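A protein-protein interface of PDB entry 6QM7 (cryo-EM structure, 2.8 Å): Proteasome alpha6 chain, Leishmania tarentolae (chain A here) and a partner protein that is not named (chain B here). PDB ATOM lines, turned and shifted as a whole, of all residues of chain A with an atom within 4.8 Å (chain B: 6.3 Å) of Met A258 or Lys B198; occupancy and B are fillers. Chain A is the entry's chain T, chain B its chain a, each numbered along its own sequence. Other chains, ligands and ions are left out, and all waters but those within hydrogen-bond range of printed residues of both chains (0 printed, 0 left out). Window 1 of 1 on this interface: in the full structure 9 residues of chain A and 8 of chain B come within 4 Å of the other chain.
Hydrophobic or aromatic side chains of chain B that line the printed part of chain A: Tyr B195, Trp B199 and Tyr B202. Along chain A the printed residues that touch a printed residue of chain B span positions 230 to 262. Among the printed residues, 14 pairs touch across the chains.
Among the printed residues, pairs that only touch across the chains: Thr A255 with Trp B199, Arg A261 with Tyr B195, Met A258 with Tyr B195, Arg A254 with Tyr B202, Met A258 with Tyr B202, Arg A254 with Trp B199, Met A258 with Lys B198, Arg A261 with Lys B194 and Asp A232 with Tyr B202.
The side-chain hydroxyl (OH) of Tyr B195 sits at hydrogen-bond distance from the backbone NH (N) of Tyr A262, 3.2 Å away. OE2 of Glu A230 lies within salt-bridge range of NZ of Lys B198 (3.1 Å). NZ of Lys B198 lies within salt-bridge range of OD2 of Asp A232, at 3.9 Å. The side-chain sulfur (SD) of Met A258 sits at hydrogen-bond distance from the indole nitrogen (NE1) of Trp B199. The side-chain carboxylate of Glu A230 is in hydrogen-bond range of the side-chain hydroxyl of Tyr B202, at 3.5 Å.
Of the printed residues of chain B, Glu A230 touches Lys B198 (3.1 Å) and Tyr B202 (3.5 Å). Glu A256 touches none of the printed residues of chain B. Of chain B, only Tyr B195 (3.5 Å), Lys B198 (3.6 Å), Trp B199 (3.3 Å) and Tyr B202 (3.6 Å) come within 4 Å of Met A258. Lys B198 touches just these residues of chain A: Glu A230 (3.1 Å), Asp A232 (3.9 Å) and Met A258 (3.6 Å). Printed residues of chain A within 4 Å of Tyr B202: Glu A230 (3.5 Å), Asp A232 (3.98 Å), Arg A254 (3.6 Å) and Met A258 (3.6 Å). The nearest printed residue of chain B that does not touch Arg A261 is Lys B198 (6.3 Å).
The side-chain amino group (NZ) of Lys B198 is in hydrogen-bond range of the side-chain hydroxyl (OH) of Tyr B202. O of Trp B199 lies within hydrogen-bond range of ND2 of Asn B203 (3.1 Å). The backbone carbonyl oxygen (O) of Glu A230 lies within hydrogen-bond range of the guanidinium group (NE) of Arg A254 (2.8 Å). The guanidinium group (NE) of Arg A261 lies within salt-bridge range of the side-chain carboxylate (OD1) of Asp A232 (2.6 Å). The side-chain carboxylate of Glu A233 is in salt-bridge range of the guanidinium group of Arg A261, at 3.5 Å. The side-chain amide nitrogen (ND2) of Asn A259 sits at hydrogen-bond distance from the backbone carbonyl oxygen (O) of Thr A255 (2.9 Å).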
ATOM      1  N   GLU A 230      12.471  37.079 -23.419  1.00  0.00           N
ATOM      2  CA  GLU A 230      12.828  35.899 -24.240  1.00  0.00           C
ATOM      3  C   GLU A 230      13.282  34.854 -23.221  1.00  0.00           C
ATOM      4  O   GLU A 230      13.937  35.241 -22.230  1.00  0.00           O
ATOM      5  CB  GLU A 230      13.805  36.281 -25.362  1.00  0.00           C
ATOM      6  CG  GLU A 230      15.101  35.471 -25.425  1.00  0.00           C
ATOM      7  CD  GLU A 230      15.416  34.661 -26.677  1.00  0.00           C
ATOM      8  OE1 GLU A 230      14.555  34.583 -27.601  1.00  0.00           O
ATOM      9  OE2 GLU A 230      16.543  34.106 -26.732  1.00  0.00           O
ATOM     10  N   ASP A 232      13.769  31.235 -24.542  1.00  0.00           N
ATOM     11  CA  ASP A 232      14.648  30.511 -25.485  1.00  0.00           C
ATOM     12  C   ASP A 232      14.289  30.978 -26.888  1.00  0.00           C
ATOM     13  O   ASP A 232      13.335  31.760 -27.012  1.00  0.00           O
ATOM     14  CB  ASP A 232      14.468  29.001 -25.333  1.00  0.00           C
ATOM     15  CG  ASP A 232      15.679  28.152 -25.699  1.00  0.00           C
ATOM     16  OD1 ASP A 232      15.455  27.014 -26.161  1.00  0.00           O
ATOM     17  OD2 ASP A 232      16.836  28.611 -25.487  1.00  0.00           O
ATOM     18  N   GLU A 233      15.010  30.503 -27.903  1.00  0.00           N
ATOM     19  CA  GLU A 233      14.716  30.826 -29.326  1.00  0.00           C
ATOM     20  C   GLU A 233      13.196  30.845 -29.526  1.00  0.00           C
ATOM     21  O   GLU A 233      12.690  31.815 -30.090  1.00  0.00           O
ATOM     22  CB  GLU A 233      15.379  29.806 -30.264  1.00  0.00           C
ATOM     23  CG  GLU A 233      16.893  29.939 -30.358  1.00  0.00           C
ATOM     24  CD  GLU A 233      17.650  28.646 -30.648  1.00  0.00           C
ATOM     25  OE1 GLU A 233      18.441  28.204 -29.769  1.00  0.00           O
ATOM     26  OE2 GLU A 233      17.466  28.087 -31.758  1.00  0.00           O
ATOM     27  N   ARG A 254      14.189  29.975 -18.123  1.00  0.00           N
ATOM     28  CA  ARG A 254      15.421  30.101 -18.940  1.00  0.00           C
ATOM     29  C   ARG A 254      16.379  28.954 -18.623  1.00  0.00           C
ATOM     30  O   ARG A 254      16.879  28.323 -19.569  1.00  0.00           O
ATOM     31  CB  ARG A 254      16.104  31.441 -18.707  1.00  0.00           C
ATOM     32  CG  ARG A 254      15.458  32.542 -19.520  1.00  0.00           C
ATOM     33  CD  ARG A 254      15.694  33.890 -18.887  1.00  0.00           C
ATOM     34  NE  ARG A 254      15.351  34.969 -19.784  1.00  0.00           N
ATOM     35  CZ  ARG A 254      15.495  36.230 -19.465  1.00  0.00           C
ATOM     36  NH1 ARG A 254      15.953  36.572 -18.272  1.00  0.00           N
ATOM     37  NH2 ARG A 254      15.189  37.156 -20.342  1.00  0.00           N
ATOM     38  N   THR A 255      16.591  28.707 -17.334  1.00  0.00           N
ATOM     39  CA  THR A 255      17.466  27.634 -16.827  1.00  0.00           C
ATOM     40  C   THR A 255      16.952  26.279 -17.312  1.00  0.00           C
ATOM     41  O   THR A 255      17.784  25.487 -17.794  1.00  0.00           O
ATOM     42  CB  THR A 255      17.567  27.672 -15.308  1.00  0.00           C
ATOM     43  OG1 THR A 255      18.075  28.966 -14.984  1.00  0.00           O
ATOM     44  CG2 THR A 255      18.461  26.574 -14.768  1.00  0.00           C
ATOM     45  N   GLU A 256      15.652  26.016 -17.189  1.00  0.00           N
ATOM     46  CA  GLU A 256      15.066  24.702 -17.559  1.00  0.00           C
ATOM     47  C   GLU A 256      15.086  24.540 -19.076  1.00  0.00           C
ATOM     48  O   GLU A 256      15.322  23.405 -19.523  1.00  0.00           O
ATOM     49  CB  GLU A 256      13.646  24.540 -17.018  1.00  0.00           C
ATOM     50  CG  GLU A 256      13.590  24.345 -15.506  1.00  0.00           C
ATOM     51  CD  GLU A 256      14.425  23.200 -14.950  1.00  0.00           C
ATOM     52  OE1 GLU A 256      14.473  22.132 -15.604  1.00  0.00           O
ATOM     53  OE2 GLU A 256      15.047  23.386 -13.876  1.00  0.00           O
ATOM     54  N   CYS A 257      14.865  25.613 -19.834  1.00  0.00           N
ATOM     55  CA  CYS A 257      14.900  25.562 -21.318  1.00  0.00           C
ATOM     56  C   CYS A 257      16.319  25.294 -21.800  1.00  0.00           C
ATOM     57  O   CYS A 257      16.460  24.577 -22.788  1.00  0.00           O
ATOM     58  CB  CYS A 257      14.341  26.824 -21.953  1.00  0.00           C
ATOM     59  SG  CYS A 257      12.539  26.841 -21.853  1.00  0.00           S
ATOM     60  N   MET A 258      17.322  25.845 -21.122  1.00  0.00           N
ATOM     61  CA  MET A 258      18.749  25.644 -21.479  1.00  0.00           C
ATOM     62  C   MET A 258      19.082  24.188 -21.220  1.00  0.00           C
ATOM     63  O   MET A 258      19.538  23.540 -22.147  1.00  0.00           O
ATOM     64  CB  MET A 258      19.690  26.525 -20.657  1.00  0.00           C
ATOM     65  CG  MET A 258      19.762  27.945 -21.182  1.00  0.00           C
ATOM     66  SD  MET A 258      20.794  28.976 -20.135  1.00  0.00           S
ATOM     67  CE  MET A 258      20.103  30.590 -20.472  1.00  0.00           C
ATOM     68  N   ASN A 259      18.845  23.721 -20.001  1.00  0.00           N
ATOM     69  CA  ASN A 259      18.975  22.298 -19.618  1.00  0.00           C
ATOM     70  C   ASN A 259      18.350  21.421 -20.693  1.00  0.00           C
ATOM     71  O   ASN A 259      19.034  20.504 -21.186  1.00  0.00           O
ATOM     72  CB  ASN A 259      18.286  22.005 -18.289  1.00  0.00           C
ATOM     73  CG  ASN A 259      19.228  22.234 -17.134  1.00  0.00           C
ATOM     74  OD1 ASN A 259      20.220  21.518 -17.021  1.00  0.00           O
ATOM     75  ND2 ASN A 259      18.948  23.228 -16.304  1.00  0.00           N
ATOM     76  N   TYR A 260      17.095  21.679 -21.037  1.00  0.00           N
ATOM     77  CA  TYR A 260      16.383  20.844 -22.030  1.00  0.00           C
ATOM     78  C   TYR A 260      17.189  20.874 -23.320  1.00  0.00           C
ATOM     79  O   TYR A 260      17.620  19.809 -23.756  1.00  0.00           O
ATOM     80  CB  TYR A 260      14.932  21.278 -22.232  1.00  0.00           C
ATOM     81  CG  TYR A 260      14.174  20.318 -23.107  1.00  0.00           C
ATOM     82  CD1 TYR A 260      13.409  19.299 -22.569  1.00  0.00           C
ATOM     83  CD2 TYR A 260      14.281  20.399 -24.486  1.00  0.00           C
ATOM     84  CE1 TYR A 260      12.746  18.397 -23.385  1.00  0.00           C
ATOM     85  CE2 TYR A 260      13.616  19.516 -25.316  1.00  0.00           C
ATOM     86  CZ  TYR A 260      12.860  18.496 -24.765  1.00  0.00           C
ATOM     87  OH  TYR A 260      12.222  17.635 -25.616  1.00  0.00           O
ATOM     88  N   ARG A 261      17.460  22.064 -23.845  1.00  0.00           N
ATOM     89  CA  ARG A 261      18.193  22.251 -25.128  1.00  0.00           C
ATOM     90  C   ARG A 261      19.591  21.630 -25.073  1.00  0.00           C
ATOM     91  O   ARG A 261      20.036  21.115 -26.082  1.00  0.00           O
ATOM     92  CB  ARG A 261      18.282  23.732 -25.485  1.00  0.00           C
ATOM     93  CG  ARG A 261      18.657  23.973 -26.937  1.00  0.00           C
ATOM     94  CD  ARG A 261      18.520  25.437 -27.274  1.00  0.00           C
ATOM     95  NE  ARG A 261      17.146  25.765 -27.606  1.00  0.00           N
ATOM     96  CZ  ARG A 261      16.540  25.478 -28.755  1.00  0.00           C
ATOM     97  NH1 ARG A 261      17.185  24.820 -29.709  1.00  0.00           N
ATOM     98  NH2 ARG A 261      15.283  25.855 -28.946  1.00  0.00           N
ATOM     99  N   TYR A 262      20.256  21.693 -23.931  1.00  0.00           N
ATOM    100  CA  TYR A 262      21.566  21.044 -23.701  1.00  0.00           C
ATOM    101  C   TYR A 262      21.415  19.542 -23.911  1.00  0.00           C
ATOM    102  O   TYR A 262      22.214  18.964 -24.682  1.00  0.00           O
ATOM    103  CB  TYR A 262      22.099  21.317 -22.300  1.00  0.00           C
ATOM    104  CG  TYR A 262      23.300  20.479 -21.950  1.00  0.00           C
ATOM    105  CD1 TYR A 262      24.509  20.645 -22.610  1.00  0.00           C
ATOM    106  CD2 TYR A 262      23.225  19.493 -20.982  1.00  0.00           C
ATOM    107  CE1 TYR A 262      25.611  19.864 -22.301  1.00  0.00           C
ATOM    108  CE2 TYR A 262      24.323  18.715 -20.655  1.00  0.00           C
ATOM    109  CZ  TYR A 262      25.519  18.901 -21.315  1.00  0.00           C
ATOM    110  OH  TYR A 262      26.591  18.119 -21.007  1.00  0.00           O
ATOM    111  N   LEU B 193      29.884  27.446 -22.963  1.00  0.00           N
ATOM    112  CA  LEU B 193      30.062  28.850 -23.394  1.00  0.00           C
ATOM    113  C   LEU B 193      28.775  29.356 -24.004  1.00  0.00           C
ATOM    114  O   LEU B 193      28.467  30.510 -23.762  1.00  0.00           O
ATOM    115  CB  LEU B 193      31.195  28.951 -24.404  1.00  0.00           C
ATOM    116  CG  LEU B 193      32.533  29.174 -23.732  1.00  0.00           C
ATOM    117  CD1 LEU B 193      33.652  28.450 -24.448  1.00  0.00           C
ATOM    118  CD2 LEU B 193      32.796  30.659 -23.644  1.00  0.00           C
ATOM    119  N   LYS B 194      28.091  28.533 -24.787  1.00  0.00           N
ATOM    120  CA  LYS B 194      26.822  28.920 -25.438  1.00  0.00           C
ATOM    121  C   LYS B 194      25.857  29.455 -24.384  1.00  0.00           C
ATOM    122  O   LYS B 194      25.172  30.439 -24.680  1.00  0.00           O
ATOM    123  CB  LYS B 194      26.185  27.739 -26.166  1.00  0.00           C
ATOM    124  CG  LYS B 194      24.900  28.099 -26.890  1.00  0.00           C
ATOM    125  CD  LYS B 194      24.201  26.951 -27.553  1.00  0.00           C
ATOM    126  CE  LYS B 194      22.785  27.336 -27.927  1.00  0.00           C
ATOM    127  NZ  LYS B 194      22.011  26.163 -28.391  1.00  0.00           N
ATOM    128  N   TYR B 195      25.814  28.820 -23.213  1.00  0.00           N
ATOM    129  CA  TYR B 195      24.851  29.118 -22.126  1.00  0.00           C
ATOM    130  C   TYR B 195      25.369  30.286 -21.294  1.00  0.00           C
ATOM    131  O   TYR B 195      24.537  31.099 -20.895  1.00  0.00           O
ATOM    132  CB  TYR B 195      24.468  27.829 -21.383  1.00  0.00           C
ATOM    133  CG  TYR B 195      23.707  26.890 -22.296  1.00  0.00           C
ATOM    134  CD1 TYR B 195      22.639  27.344 -23.073  1.00  0.00           C
ATOM    135  CD2 TYR B 195      24.098  25.569 -22.471  1.00  0.00           C
ATOM    136  CE1 TYR B 195      21.973  26.518 -23.970  1.00  0.00           C
ATOM    137  CE2 TYR B 195      23.447  24.733 -23.371  1.00  0.00           C
ATOM    138  CZ  TYR B 195      22.378  25.203 -24.121  1.00  0.00           C
ATOM    139  OH  TYR B 195      21.734  24.371 -24.994  1.00  0.00           O
ATOM    140  N   ARG B 196      26.674  30.422 -21.098  1.00  0.00           N
ATOM    141  CA  ARG B 196      27.234  31.621 -20.429  1.00  0.00           C
ATOM    142  C   ARG B 196      26.960  32.850 -21.290  1.00  0.00           C
ATOM    143  O   ARG B 196      26.701  33.914 -20.721  1.00  0.00           O
ATOM    144  CB  ARG B 196      28.720  31.448 -20.138  1.00  0.00           C
ATOM    145  CG  ARG B 196      29.003  30.510 -18.975  1.00  0.00           C
ATOM    146  CD  ARG B 196      28.681  31.132 -17.629  1.00  0.00           C
ATOM    147  NE  ARG B 196      29.868  31.077 -16.774  1.00  0.00           N
ATOM    148  CZ  ARG B 196      30.590  32.123 -16.345  1.00  0.00           C
ATOM    149  NH1 ARG B 196      30.259  33.375 -16.647  1.00  0.00           N
ATOM    150  NH2 ARG B 196      31.647  31.903 -15.580  1.00  0.00           N
ATOM    151  N   VAL B 197      27.006  32.698 -22.606  1.00  0.00           N
ATOM    152  CA  VAL B 197      26.792  33.804 -23.579  1.00  0.00           C
ATOM    153  C   VAL B 197      25.306  34.124 -23.610  1.00  0.00           C
ATOM    154  O   VAL B 197      24.969  35.297 -23.817  1.00  0.00           O
ATOM    155  CB  VAL B 197      27.329  33.444 -24.977  1.00  0.00           C
ATOM    156  CG1 VAL B 197      26.866  34.418 -26.046  1.00  0.00           C
ATOM    157  CG2 VAL B 197      28.843  33.353 -24.981  1.00  0.00           C
ATOM    158  N   LYS B 198      24.454  33.120 -23.442  1.00  0.00           N
ATOM    159  CA  LYS B 198      22.981  33.299 -23.451  1.00  0.00           C
ATOM    160  C   LYS B 198      22.584  34.060 -22.189  1.00  0.00           C
ATOM    161  O   LYS B 198      21.796  34.986 -22.302  1.00  0.00           O
ATOM    162  CB  LYS B 198      22.290  31.944 -23.585  1.00  0.00           C
ATOM    163  CG  LYS B 198      20.782  31.999 -23.758  1.00  0.00           C
ATOM    164  CD  LYS B 198      20.238  31.118 -24.886  1.00  0.00           C
ATOM    165  CE  LYS B 198      20.020  31.893 -26.174  1.00  0.00           C
ATOM    166  NZ  LYS B 198      18.601  31.855 -26.614  1.00  0.00           N
ATOM    167  N   TRP B 199      23.160  33.714 -21.042  1.00  0.00           N
ATOM    168  CA  TRP B 199      22.925  34.411 -19.751  1.00  0.00           C
ATOM    169  C   TRP B 199      23.382  35.852 -19.861  1.00  0.00           C
ATOM    170  O   TRP B 199      22.671  36.735 -19.391  1.00  0.00           O
ATOM    171  CB  TRP B 199      23.636  33.717 -18.588  1.00  0.00           C
ATOM    172  CG  TRP B 199      22.870  32.539 -18.095  1.00  0.00           C
ATOM    173  CD1 TRP B 199      23.260  31.233 -18.062  1.00  0.00           C
ATOM    174  CD2 TRP B 199      21.518  32.573 -17.631  1.00  0.00           C
ATOM    175  NE1 TRP B 199      22.246  30.453 -17.579  1.00  0.00           N
ATOM    176  CE2 TRP B 199      21.164  31.248 -17.309  1.00  0.00           C
ATOM    177  CE3 TRP B 199      20.591  33.599 -17.439  1.00  0.00           C
ATOM    178  CZ2 TRP B 199      19.911  30.922 -16.802  1.00  0.00           C
ATOM    179  CZ3 TRP B 199      19.348  33.276 -16.949  1.00  0.00           C
ATOM    180  CH2 TRP B 199      19.015  31.954 -16.639  1.00  0.00           C
ATOM    181  N   TYR B 200      24.550  36.072 -20.425  1.00  0.00           N
ATOM    182  CA  TYR B 200      25.075  37.433 -20.641  1.00  0.00           C
ATOM    183  C   TYR B 200      24.031  38.217 -21.435  1.00  0.00           C
ATOM    184  O   TYR B 200      23.752  39.330 -21.004  1.00  0.00           O
ATOM    185  CB  TYR B 200      26.461  37.358 -21.277  1.00  0.00           C
ATOM    186  CG  TYR B 200      27.136  38.686 -21.464  1.00  0.00           C
ATOM    187  CD1 TYR B 200      28.200  39.071 -20.666  1.00  0.00           C
ATOM    188  CD2 TYR B 200      26.711  39.556 -22.452  1.00  0.00           C
ATOM    189  CE1 TYR B 200      28.820  40.295 -20.843  1.00  0.00           C
ATOM    190  CE2 TYR B 200      27.314  40.784 -22.637  1.00  0.00           C
ATOM    191  CZ  TYR B 200      28.377  41.151 -21.836  1.00  0.00           C
ATOM    192  OH  TYR B 200      28.974  42.355 -22.068  1.00  0.00           O
ATOM    193  N   LYS B 201      23.446  37.660 -22.505  1.00  0.00           N
ATOM    194  CA  LYS B 201      22.428  38.377 -23.330  1.00  0.00           C
ATOM    195  C   LYS B 201      21.253  38.810 -22.453  1.00  0.00           C
ATOM    196  O   LYS B 201      20.765  39.926 -22.661  1.00  0.00           O
ATOM    197  CB  LYS B 201      21.862  37.543 -24.481  1.00  0.00           C
ATOM    198  CG  LYS B 201      22.668  37.588 -25.770  1.00  0.00           C
ATOM    199  CD  LYS B 201      22.414  36.374 -26.662  1.00  0.00           C
ATOM    200  CE  LYS B 201      22.685  36.613 -28.135  1.00  0.00           C
ATOM    201  NZ  LYS B 201      21.590  37.381 -28.776  1.00  0.00           N
ATOM    202  N   TYR B 202      20.825  37.962 -21.522  1.00  0.00           N
ATOM    203  CA  TYR B 202      19.662  38.212 -20.637  1.00  0.00           C
ATOM    204  C   TYR B 202      20.011  39.264 -19.574  1.00  0.00           C
ATOM    205  O   TYR B 202      19.275  40.265 -19.456  1.00  0.00           O
ATOM    206  CB  TYR B 202      19.186  36.900 -20.014  1.00  0.00           C
ATOM    207  CG  TYR B 202      18.690  35.848 -20.980  1.00  0.00           C
ATOM    208  CD1 TYR B 202      18.069  36.181 -22.176  1.00  0.00           C
ATOM    209  CD2 TYR B 202      18.774  34.500 -20.657  1.00  0.00           C
ATOM    210  CE1 TYR B 202      17.589  35.207 -23.035  1.00  0.00           C
ATOM    211  CE2 TYR B 202      18.301  33.511 -21.505  1.00  0.00           C
ATOM    212  CZ  TYR B 202      17.708  33.864 -22.706  1.00  0.00           C
ATOM    213  OH  TYR B 202      17.252  32.888 -23.556  1.00  0.00           O
ATOM    214  N   ASN B 203      21.122  39.084 -18.867  1.00  0.00           N
ATOM    215  CA  ASN B 203      21.551  39.975 -17.756  1.00  0.00           C
ATOM    216  C   ASN B 203      22.057  41.323 -18.295  1.00  0.00           C
ATOM    217  O   ASN B 203      22.050  42.283 -17.514  1.00  0.00           O
ATOM    218  CB  ASN B 203      22.600  39.313 -16.855  1.00  0.00           C
ATOM    219  CG  ASN B 203      22.178  37.949 -16.348  1.00  0.00           C
ATOM    220  OD1 ASN B 203      21.026  37.746 -15.979  1.00  0.00           O
ATOM    221  ND2 ASN B 203      23.102  37.002 -16.331  1.00  0.00           N
